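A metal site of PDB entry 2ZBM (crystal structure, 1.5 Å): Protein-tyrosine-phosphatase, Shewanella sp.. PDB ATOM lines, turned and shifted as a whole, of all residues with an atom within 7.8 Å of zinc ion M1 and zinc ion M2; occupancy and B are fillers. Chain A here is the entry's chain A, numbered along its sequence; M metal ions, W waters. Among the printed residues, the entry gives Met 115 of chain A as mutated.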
ATOM      1  N   SER A  77       6.283  34.477 -23.627  1.00  0.00           N
ATOM      2  CA  SER A  77       6.409  33.062 -24.015  1.00  0.00           C
ATOM      3  C   SER A  77       5.505  32.664 -25.161  1.00  0.00           C
ATOM      4  O   SER A  77       4.544  33.419 -25.383  1.00  0.00           O
ATOM      5  CB  SER A  77       6.022  32.163 -22.821  1.00  0.00           C
ATOM      6  OG  SER A  77       6.542  30.848 -22.967  1.00  0.00           O
ATOM      7  N   ASP A  78       5.779  31.533 -25.800  1.00  0.00           N
ATOM      8  CA  ASP A  78       4.774  30.914 -26.684  1.00  0.00           C
ATOM      9  C   ASP A  78       4.325  31.882 -27.782  1.00  0.00           C
ATOM     10  O   ASP A  78       3.148  32.016 -28.106  1.00  0.00           O
ATOM     11  CB  ASP A  78       3.567  30.342 -25.896  1.00  0.00           C
ATOM     12  CG  ASP A  78       4.001  29.223 -24.971  1.00  0.00           C
ATOM     13  OD1 ASP A  78       3.923  28.035 -25.339  1.00  0.00           O
ATOM     14  OD2 ASP A  78       4.442  29.571 -23.813  1.00  0.00           O
ATOM     15  N   VAL A  79       5.327  32.517 -28.411  1.00  0.00           N
ATOM     16  CA  VAL A  79       5.022  33.382 -29.571  1.00  0.00           C
ATOM     17  C   VAL A  79       4.480  32.566 -30.732  1.00  0.00           C
ATOM     18  O   VAL A  79       3.620  33.051 -31.507  1.00  0.00           O
ATOM     19  CB  VAL A  79       6.308  34.148 -29.956  1.00  0.00           C
ATOM     20  CG1 VAL A  79       6.159  34.855 -31.294  1.00  0.00           C
ATOM     21  CG2 VAL A  79       6.685  35.147 -28.849  1.00  0.00           C
ATOM     22  N   HIS A  80       4.904  31.306 -30.893  1.00  0.00           N
ATOM     23  CA  HIS A  80       4.344  30.404 -31.915  1.00  0.00           C
ATOM     24  C   HIS A  80       4.251  31.047 -33.288  1.00  0.00           C
ATOM     25  O   HIS A  80       3.163  31.095 -33.910  1.00  0.00           O
ATOM     26  CB  HIS A  80       2.972  29.829 -31.410  1.00  0.00           C
ATOM     27  CG  HIS A  80       3.168  28.738 -30.397  1.00  0.00           C
ATOM     28  ND1 HIS A  80       3.914  27.592 -30.665  1.00  0.00           N
ATOM     29  CD2 HIS A  80       2.734  28.596 -29.098  1.00  0.00           C
ATOM     30  CE1 HIS A  80       3.900  26.834 -29.586  1.00  0.00           C
ATOM     31  NE2 HIS A  80       3.204  27.403 -28.613  1.00  0.00           N
ATOM     32  N   THR A 112      10.326  32.234 -22.505  1.00  0.00           N
ATOM     33  CA  THR A 112      10.317  30.890 -21.953  1.00  0.00           C
ATOM     34  C   THR A 112       9.820  29.858 -22.955  1.00  0.00           C
ATOM     35  O   THR A 112       8.967  29.036 -22.562  1.00  0.00           O
ATOM     36  CB  THR A 112       9.498  30.804 -20.646  1.00  0.00           C
ATOM     37  OG1 THR A 112       8.169  31.280 -20.871  1.00  0.00           O
ATOM     38  CG2 THR A 112      10.100  31.724 -19.576  1.00  0.00           C
ATOM     39  N   GLY A 113      10.311  29.866 -24.209  1.00  0.00           N
ATOM     40  CA  GLY A 113      10.098  28.789 -25.133  1.00  0.00           C
ATOM     41  C   GLY A 113       8.975  29.001 -26.148  1.00  0.00           C
ATOM     42  O   GLY A 113       8.195  29.965 -26.077  1.00  0.00           O
ATOM     43  N   ASP A 114       8.895  28.052 -27.094  1.00  0.00           N
ATOM     44  CA  ASP A 114       7.847  27.941 -28.088  1.00  0.00           C
ATOM     45  C   ASP A 114       7.755  29.142 -29.028  1.00  0.00           C
ATOM     46  O   ASP A 114       6.674  29.748 -29.262  1.00  0.00           O
ATOM     47  CB  ASP A 114       6.482  27.688 -27.409  1.00  0.00           C
ATOM     48  CG  ASP A 114       6.268  26.208 -27.127  1.00  0.00           C
ATOM     49  OD1 ASP A 114       5.148  25.839 -26.733  1.00  0.00           O
ATOM     50  OD2 ASP A 114       7.246  25.419 -27.204  1.00  0.00           O
ATOM     51  N   MET A 115       8.901  29.403 -29.644  1.00  0.00           N
ATOM     52  CA  MET A 115       8.960  30.323 -30.751  1.00  0.00           C
ATOM     53  C   MET A 115       8.417  29.646 -32.029  1.00  0.00           C
ATOM     54  O   MET A 115       7.761  30.305 -32.864  1.00  0.00           O
ATOM     55  CB  MET A 115      10.368  30.835 -31.073  1.00  0.00           C
ATOM     56  CG  MET A 115      10.910  31.777 -29.974  1.00  0.00           C
ATOM     57  SD  MET A 115      12.666  32.128 -30.242  1.00  0.00           S
ATOM     58  CE  MET A 115      13.384  30.516 -29.893  1.00  0.00           C
ATOM     59  N   PHE A 116       8.689  28.337 -32.167  1.00  0.00           N
ATOM     60  CA  PHE A 116       8.262  27.605 -33.331  1.00  0.00           C
ATOM     61  C   PHE A 116       6.786  27.216 -33.324  1.00  0.00           C
ATOM     62  O   PHE A 116       6.181  27.167 -32.249  1.00  0.00           O
ATOM     63  CB  PHE A 116       9.007  26.277 -33.373  1.00  0.00           C
ATOM     64  CG  PHE A 116      10.436  26.408 -33.862  1.00  0.00           C
ATOM     65  CD1 PHE A 116      11.481  26.621 -32.950  1.00  0.00           C
ATOM     66  CD2 PHE A 116      10.706  26.302 -35.214  1.00  0.00           C
ATOM     67  CE1 PHE A 116      12.771  26.719 -33.423  1.00  0.00           C
ATOM     68  CE2 PHE A 116      12.001  26.378 -35.686  1.00  0.00           C
ATOM     69  CZ  PHE A 116      13.056  26.543 -34.795  1.00  0.00           C
ATOM     70  N   ASP A 117       6.240  26.859 -34.456  1.00  0.00           N
ATOM     71  CA  ASP A 117       5.038  26.100 -34.692  1.00  0.00           C
ATOM     72  C   ASP A 117       3.768  26.966 -34.576  1.00  0.00           C
ATOM     73  O   ASP A 117       3.741  28.026 -33.951  1.00  0.00           O
ATOM     74  CB  ASP A 117       4.975  24.862 -33.792  1.00  0.00           C
ATOM     75  CG  ASP A 117       5.904  23.734 -34.270  1.00  0.00           C
ATOM     76  OD1 ASP A 117       5.977  22.684 -33.589  1.00  0.00           O
ATOM     77  OD2 ASP A 117       6.554  23.878 -35.335  1.00  0.00           O
ATOM     78  N   GLY A 148      11.492  25.440 -25.427  1.00  0.00           N
ATOM     79  CA  GLY A 148      10.135  24.965 -25.050  1.00  0.00           C
ATOM     80  C   GLY A 148       9.914  23.593 -25.684  1.00  0.00           C
ATOM     81  O   GLY A 148      10.785  23.010 -26.397  1.00  0.00           O
ATOM     82  N   ASN A 149       8.735  23.014 -25.508  1.00  0.00           N
ATOM     83  CA  ASN A 149       8.475  21.687 -26.068  1.00  0.00           C
ATOM     84  C   ASN A 149       8.466  21.774 -27.606  1.00  0.00           C
ATOM     85  O   ASN A 149       8.906  20.799 -28.228  1.00  0.00           O
ATOM     86  CB  ASN A 149       7.206  21.031 -25.497  1.00  0.00           C
ATOM     87  CG  ASN A 149       5.913  21.721 -25.835  1.00  0.00           C
ATOM     88  OD1 ASN A 149       4.931  21.096 -26.282  1.00  0.00           O
ATOM     89  ND2 ASN A 149       5.887  23.020 -25.599  1.00  0.00           N
ATOM     90  N   HIS A 150       8.045  22.884 -28.196  1.00  0.00           N
ATOM     91  CA  HIS A 150       8.061  22.899 -29.683  1.00  0.00           C
ATOM     92  C   HIS A 150       9.480  23.064 -30.236  1.00  0.00           C
ATOM     93  O   HIS A 150       9.779  22.500 -31.329  1.00  0.00           O
ATOM     94  CB  HIS A 150       7.156  24.004 -30.163  1.00  0.00           C
ATOM     95  CG  HIS A 150       5.716  23.524 -30.013  1.00  0.00           C
ATOM     96  ND1 HIS A 150       5.006  23.003 -31.077  1.00  0.00           N
ATOM     97  CD2 HIS A 150       4.928  23.475 -28.930  1.00  0.00           C
ATOM     98  CE1 HIS A 150       3.772  22.655 -30.615  1.00  0.00           C
ATOM     99  NE2 HIS A 150       3.696  22.939 -29.321  1.00  0.00           N
ATOM    100  N   GLU A 151      10.367  23.767 -29.541  1.00  0.00           N
ATOM    101  CA  GLU A 151      11.785  23.720 -29.982  1.00  0.00           C
ATOM    102  C   GLU A 151      12.302  22.280 -30.002  1.00  0.00           C
ATOM    103  O   GLU A 151      13.006  21.863 -30.935  1.00  0.00           O
ATOM    104  CB  GLU A 151      12.732  24.578 -29.150  1.00  0.00           C
ATOM    105  CG  GLU A 151      12.667  26.068 -29.455  1.00  0.00           C
ATOM    106  CD  GLU A 151      11.338  26.671 -29.003  1.00  0.00           C
ATOM    107  OE1 GLU A 151      10.870  27.607 -29.701  1.00  0.00           O
ATOM    108  OE2 GLU A 151      10.804  26.230 -27.954  1.00  0.00           O
ATOM    109  N   MET A 153      10.549  19.501 -30.150  1.00  0.00           N
ATOM    110  CA  MET A 153       9.864  18.712 -31.202  1.00  0.00           C
ATOM    111  C   MET A 153      10.447  19.034 -32.565  1.00  0.00           C
ATOM    112  O   MET A 153      10.805  18.101 -33.321  1.00  0.00           O
ATOM    113  CB  MET A 153       8.350  18.935 -31.187  1.00  0.00           C
ATOM    114  CG  MET A 153       7.732  18.025 -30.126  1.00  0.00           C
ATOM    115  SD  MET A 153       5.953  18.064 -30.134  1.00  0.00           S
ATOM    116  CE  MET A 153       5.554  19.700 -29.514  1.00  0.00           C
ATOM    117  N   HIS A 207       9.686  26.437 -19.429  1.00  0.00           N
ATOM    118  CA  HIS A 207       8.547  26.485 -20.320  1.00  0.00           C
ATOM    119  C   HIS A 207       7.305  25.899 -19.667  1.00  0.00           C
ATOM    120  O   HIS A 207       6.247  26.577 -19.692  1.00  0.00           O
ATOM    121  CB  HIS A 207       8.923  25.691 -21.590  1.00  0.00           C
ATOM    122  CG  HIS A 207       7.767  25.748 -22.581  1.00  0.00           C
ATOM    123  ND1 HIS A 207       7.368  26.952 -23.133  1.00  0.00           N
ATOM    124  CD2 HIS A 207       6.939  24.804 -23.045  1.00  0.00           C
ATOM    125  CE1 HIS A 207       6.350  26.724 -23.905  1.00  0.00           C
ATOM    126  NE2 HIS A 207       6.039  25.421 -23.912  1.00  0.00           N
ATOM    127  N   GLY A 208       7.397  24.672 -19.127  1.00  0.00           N
ATOM    128  CA  GLY A 208       6.154  24.015 -18.648  1.00  0.00           C
ATOM    129  C   GLY A 208       5.971  24.121 -17.156  1.00  0.00           C
ATOM    130  O   GLY A 208       4.972  24.661 -16.598  1.00  0.00           O
ATOM    131  N   THR A 255       9.512  20.770 -19.767  1.00  0.00           N
ATOM    132  CA  THR A 255       8.983  21.496 -20.936  1.00  0.00           C
ATOM    133  C   THR A 255       7.581  21.027 -21.275  1.00  0.00           C
ATOM    134  O   THR A 255       7.006  21.677 -22.158  1.00  0.00           O
ATOM    135  CB  THR A 255       9.871  21.373 -22.187  1.00  0.00           C
ATOM    136  OG1 THR A 255      10.076  19.974 -22.412  1.00  0.00           O
ATOM    137  CG2 THR A 255      11.225  22.027 -21.952  1.00  0.00           C
ATOM    138  N   TRP A 256       7.028  19.993 -20.650  1.00  0.00           N
ATOM    139  CA  TRP A 256       5.654  19.616 -20.963  1.00  0.00           C
ATOM    140  C   TRP A 256       4.738  19.706 -19.763  1.00  0.00           C
ATOM    141  O   TRP A 256       3.495  19.704 -19.948  1.00  0.00           O
ATOM    142  CB  TRP A 256       5.567  18.169 -21.509  1.00  0.00           C
ATOM    143  CG  TRP A 256       6.044  17.985 -22.924  1.00  0.00           C
ATOM    144  CD1 TRP A 256       7.324  17.755 -23.368  1.00  0.00           C
ATOM    145  CD2 TRP A 256       5.215  18.004 -24.096  1.00  0.00           C
ATOM    146  NE1 TRP A 256       7.340  17.641 -24.750  1.00  0.00           N
ATOM    147  CE2 TRP A 256       6.052  17.793 -25.207  1.00  0.00           C
ATOM    148  CE3 TRP A 256       3.832  18.197 -24.229  1.00  0.00           C
ATOM    149  CZ2 TRP A 256       5.552  17.754 -26.496  1.00  0.00           C
ATOM    150  CZ3 TRP A 256       3.335  18.158 -25.508  1.00  0.00           C
ATOM    151  CH2 TRP A 256       4.172  17.947 -26.619  1.00  0.00           C
ATOM    152  N   ARG A 258       2.093  20.377 -17.044  1.00  0.00           N
ATOM    153  CA  ARG A 258       1.080  21.388 -16.889  1.00  0.00           C
ATOM    154  C   ARG A 258       0.475  21.350 -15.508  1.00  0.00           C
ATOM    155  O   ARG A 258      -0.602  21.938 -15.288  1.00  0.00           O
ATOM    156  CB  ARG A 258      -0.032  21.129 -17.934  1.00  0.00           C
ATOM    157  CG  ARG A 258       0.522  21.226 -19.365  1.00  0.00           C
ATOM    158  CD  ARG A 258      -0.645  21.348 -20.357  1.00  0.00           C
ATOM    159  NE  ARG A 258      -0.235  20.986 -21.694  1.00  0.00           N
ATOM    160  CZ  ARG A 258       0.050  21.931 -22.593  1.00  0.00           C
ATOM    161  NH1 ARG A 258       0.409  21.553 -23.794  1.00  0.00           N
ATOM    162  NH2 ARG A 258      -0.049  23.193 -22.202  1.00  0.00           N
ATOM    163  N   GLY A 285       5.414  29.220 -19.173  1.00  0.00           N
ATOM    164  CA  GLY A 285       4.589  29.444 -20.373  1.00  0.00           C
ATOM    165  C   GLY A 285       3.742  28.224 -20.639  1.00  0.00           C
ATOM    166  O   GLY A 285       3.137  27.715 -19.677  1.00  0.00           O
ATOM    167  N   HIS A 286       3.679  27.741 -21.850  1.00  0.00           N
ATOM    168  CA  HIS A 286       3.215  26.425 -22.301  1.00  0.00           C
ATOM    169  C   HIS A 286       1.696  26.239 -22.221  1.00  0.00           C
ATOM    170  O   HIS A 286       1.107  25.750 -23.212  1.00  0.00           O
ATOM    171  CB  HIS A 286       3.902  25.321 -21.494  1.00  0.00           C
ATOM    172  CG  HIS A 286       3.613  23.922 -21.965  1.00  0.00           C
ATOM    173  ND1 HIS A 286       3.779  23.413 -23.261  1.00  0.00           N
ATOM    174  CD2 HIS A 286       3.150  22.884 -21.222  1.00  0.00           C
ATOM    175  CE1 HIS A 286       3.422  22.126 -23.253  1.00  0.00           C
ATOM    176  NE2 HIS A 286       3.033  21.781 -22.017  1.00  0.00           N
ATOM    177  N   THR A 287       1.073  26.551 -21.094  1.00  0.00           N
ATOM    178  CA  THR A 287      -0.374  26.434 -20.927  1.00  0.00           C
ATOM    179  C   THR A 287      -1.046  27.803 -21.082  1.00  0.00           C
ATOM    180  O   THR A 287      -0.906  28.688 -20.225  1.00  0.00           O
ATOM    181  CB  THR A 287      -0.672  25.827 -19.543  1.00  0.00           C
ATOM    182  OG1 THR A 287       0.118  24.632 -19.408  1.00  0.00           O
ATOM    183  CG2 THR A 287      -2.133  25.439 -19.382  1.00  0.00           C
ATOM    184  N   SER A 288      -1.748  27.958 -22.234  1.00  0.00           N
ATOM    185  CA  SER A 288      -2.111  29.313 -22.651  1.00  0.00           C
ATOM    186  C   SER A 288      -3.223  29.961 -21.830  1.00  0.00           C
ATOM    187  O   SER A 288      -4.223  29.292 -21.581  1.00  0.00           O
ATOM    188  CB  SER A 288      -2.599  29.264 -24.102  1.00  0.00           C
ATOM    189  OG  SER A 288      -1.555  28.691 -24.905  1.00  0.00           O
ATOM    190  N   ASP A 304       2.342  32.526 -20.809  1.00  0.00           N
ATOM    191  CA  ASP A 304       1.743  32.198 -22.106  1.00  0.00           C
ATOM    192  C   ASP A 304       0.410  32.967 -22.162  1.00  0.00           C
ATOM    193  O   ASP A 304      -0.560  32.538 -21.507  1.00  0.00           O
ATOM    194  CB  ASP A 304       1.592  30.690 -22.372  1.00  0.00           C
ATOM    195  CG  ASP A 304       0.952  30.394 -23.731  1.00  0.00           C
ATOM    196  OD1 ASP A 304       0.888  29.217 -24.137  1.00  0.00           O
ATOM    197  OD2 ASP A 304       0.498  31.346 -24.435  1.00  0.00           O
ATOM    198  N   LYS A 308      -0.129  32.997 -29.525  1.00  0.00           N
ATOM    199  CA  LYS A 308      -0.294  32.067 -30.624  1.00  0.00           C
ATOM    200  C   LYS A 308      -1.563  32.320 -31.445  1.00  0.00           C
ATOM    201  O   LYS A 308      -1.629  31.936 -32.630  1.00  0.00           O
ATOM    202  CB  LYS A 308      -0.339  30.611 -30.105  1.00  0.00           C
ATOM    203  CG  LYS A 308      -1.594  30.299 -29.289  1.00  0.00           C
ATOM    204  CD  LYS A 308      -1.464  28.922 -28.644  1.00  0.00           C
ATOM    205  CE  LYS A 308      -2.769  28.599 -27.906  1.00  0.00           C
ATOM    206  NZ  LYS A 308      -2.758  27.340 -27.135  1.00  0.00           N
HETATM  207 ZN    ZN M   1       4.581  24.479 -24.957  1.00  0.00          ZN
HETATM  208 ZN    ZN M   2       3.181  26.850 -26.648  1.00  0.00          ZN
HETATM  209  O   HOH W   1       2.461  22.576 -26.795  1.00  0.00           O
HETATM  210  O   HOH W   2       1.280  27.578 -26.331  1.00  0.00           O
HETATM  211  O   HOH W   3       2.882  25.231 -25.714  1.00  0.00           O
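N of His 286 is in hydrogen-bond range of OD2 of Asp 78.
The side-chain carboxylate (OD2) of Asp 78 sits at hydrogen-bond distance from the side-chain hydroxyl (OG) of Ser 77 (2.6 Å).
The backbone carbonyl oxygen (O) of Thr 112 is in hydrogen-bond range of a ring nitrogen (ND1) of His 207 (2.7 Å).
The backbone carbonyl oxygen of Asp 117 lies close to a ring nitrogen (ND1) of His 80 (3.3 Å).
The backbone carbonyl oxygen of His 286 lies within hydrogen-bond range of the guanidinium group of Arg 258 (3.0 Å).
A ring nitrogen (NE2) of His 286 lies within hydrogen-bond range of the backbone carbonyl oxygen (O) of Trp 256 (3.0 Å).
OD2 of Asp 114 sits at hydrogen-bond distance from N of His 150 (2.8 Å).
The backbone NH (N) of Val 79 is in hydrogen-bond range of the backbone carbonyl oxygen (O) of Asp 114, 3.2 Å away.
Within 4 Å of zinc ion M1: Asp 78, Asp 114, Asn 149, His 207 and His 286.
The nearest printed residue that does not touch zinc ion M1 is His 150 (4.1 Å).
Within 4 Å of zinc ion M2: Asp 78, His 80 and Asp 114.
Along chain A the residues within 4 Å of zinc ion M2 span positions 78 to 114.
Zinc ion M1 is bound by water W3 (2.0 Å), NE2 of His 207 (2.0 Å), ND2 of Asn 149 (2.1 Å), ND1 of His 286 (2.2 Å) and OD1 of Asp 114 (2.3 Å).
Zinc ion M2 is bound by water W3, the side-chain carboxylate of Asp 78, a ring nitrogen (NE2) of His 80, water W2 and the side-chain carboxylate of Asp 114.
Zinc ion M2 has five donor atoms within binding distance.
Water W2 bridges the side-chain carboxylate of Asp 304 and the side-chain hydroxyl of Ser 288.
Water W1 lies within hydrogen-bond range of a ring nitrogen (NE2) of His 150 (2.8 Å) and the side-chain amide oxygen (OD1) of Asn 149 (2.9 Å).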
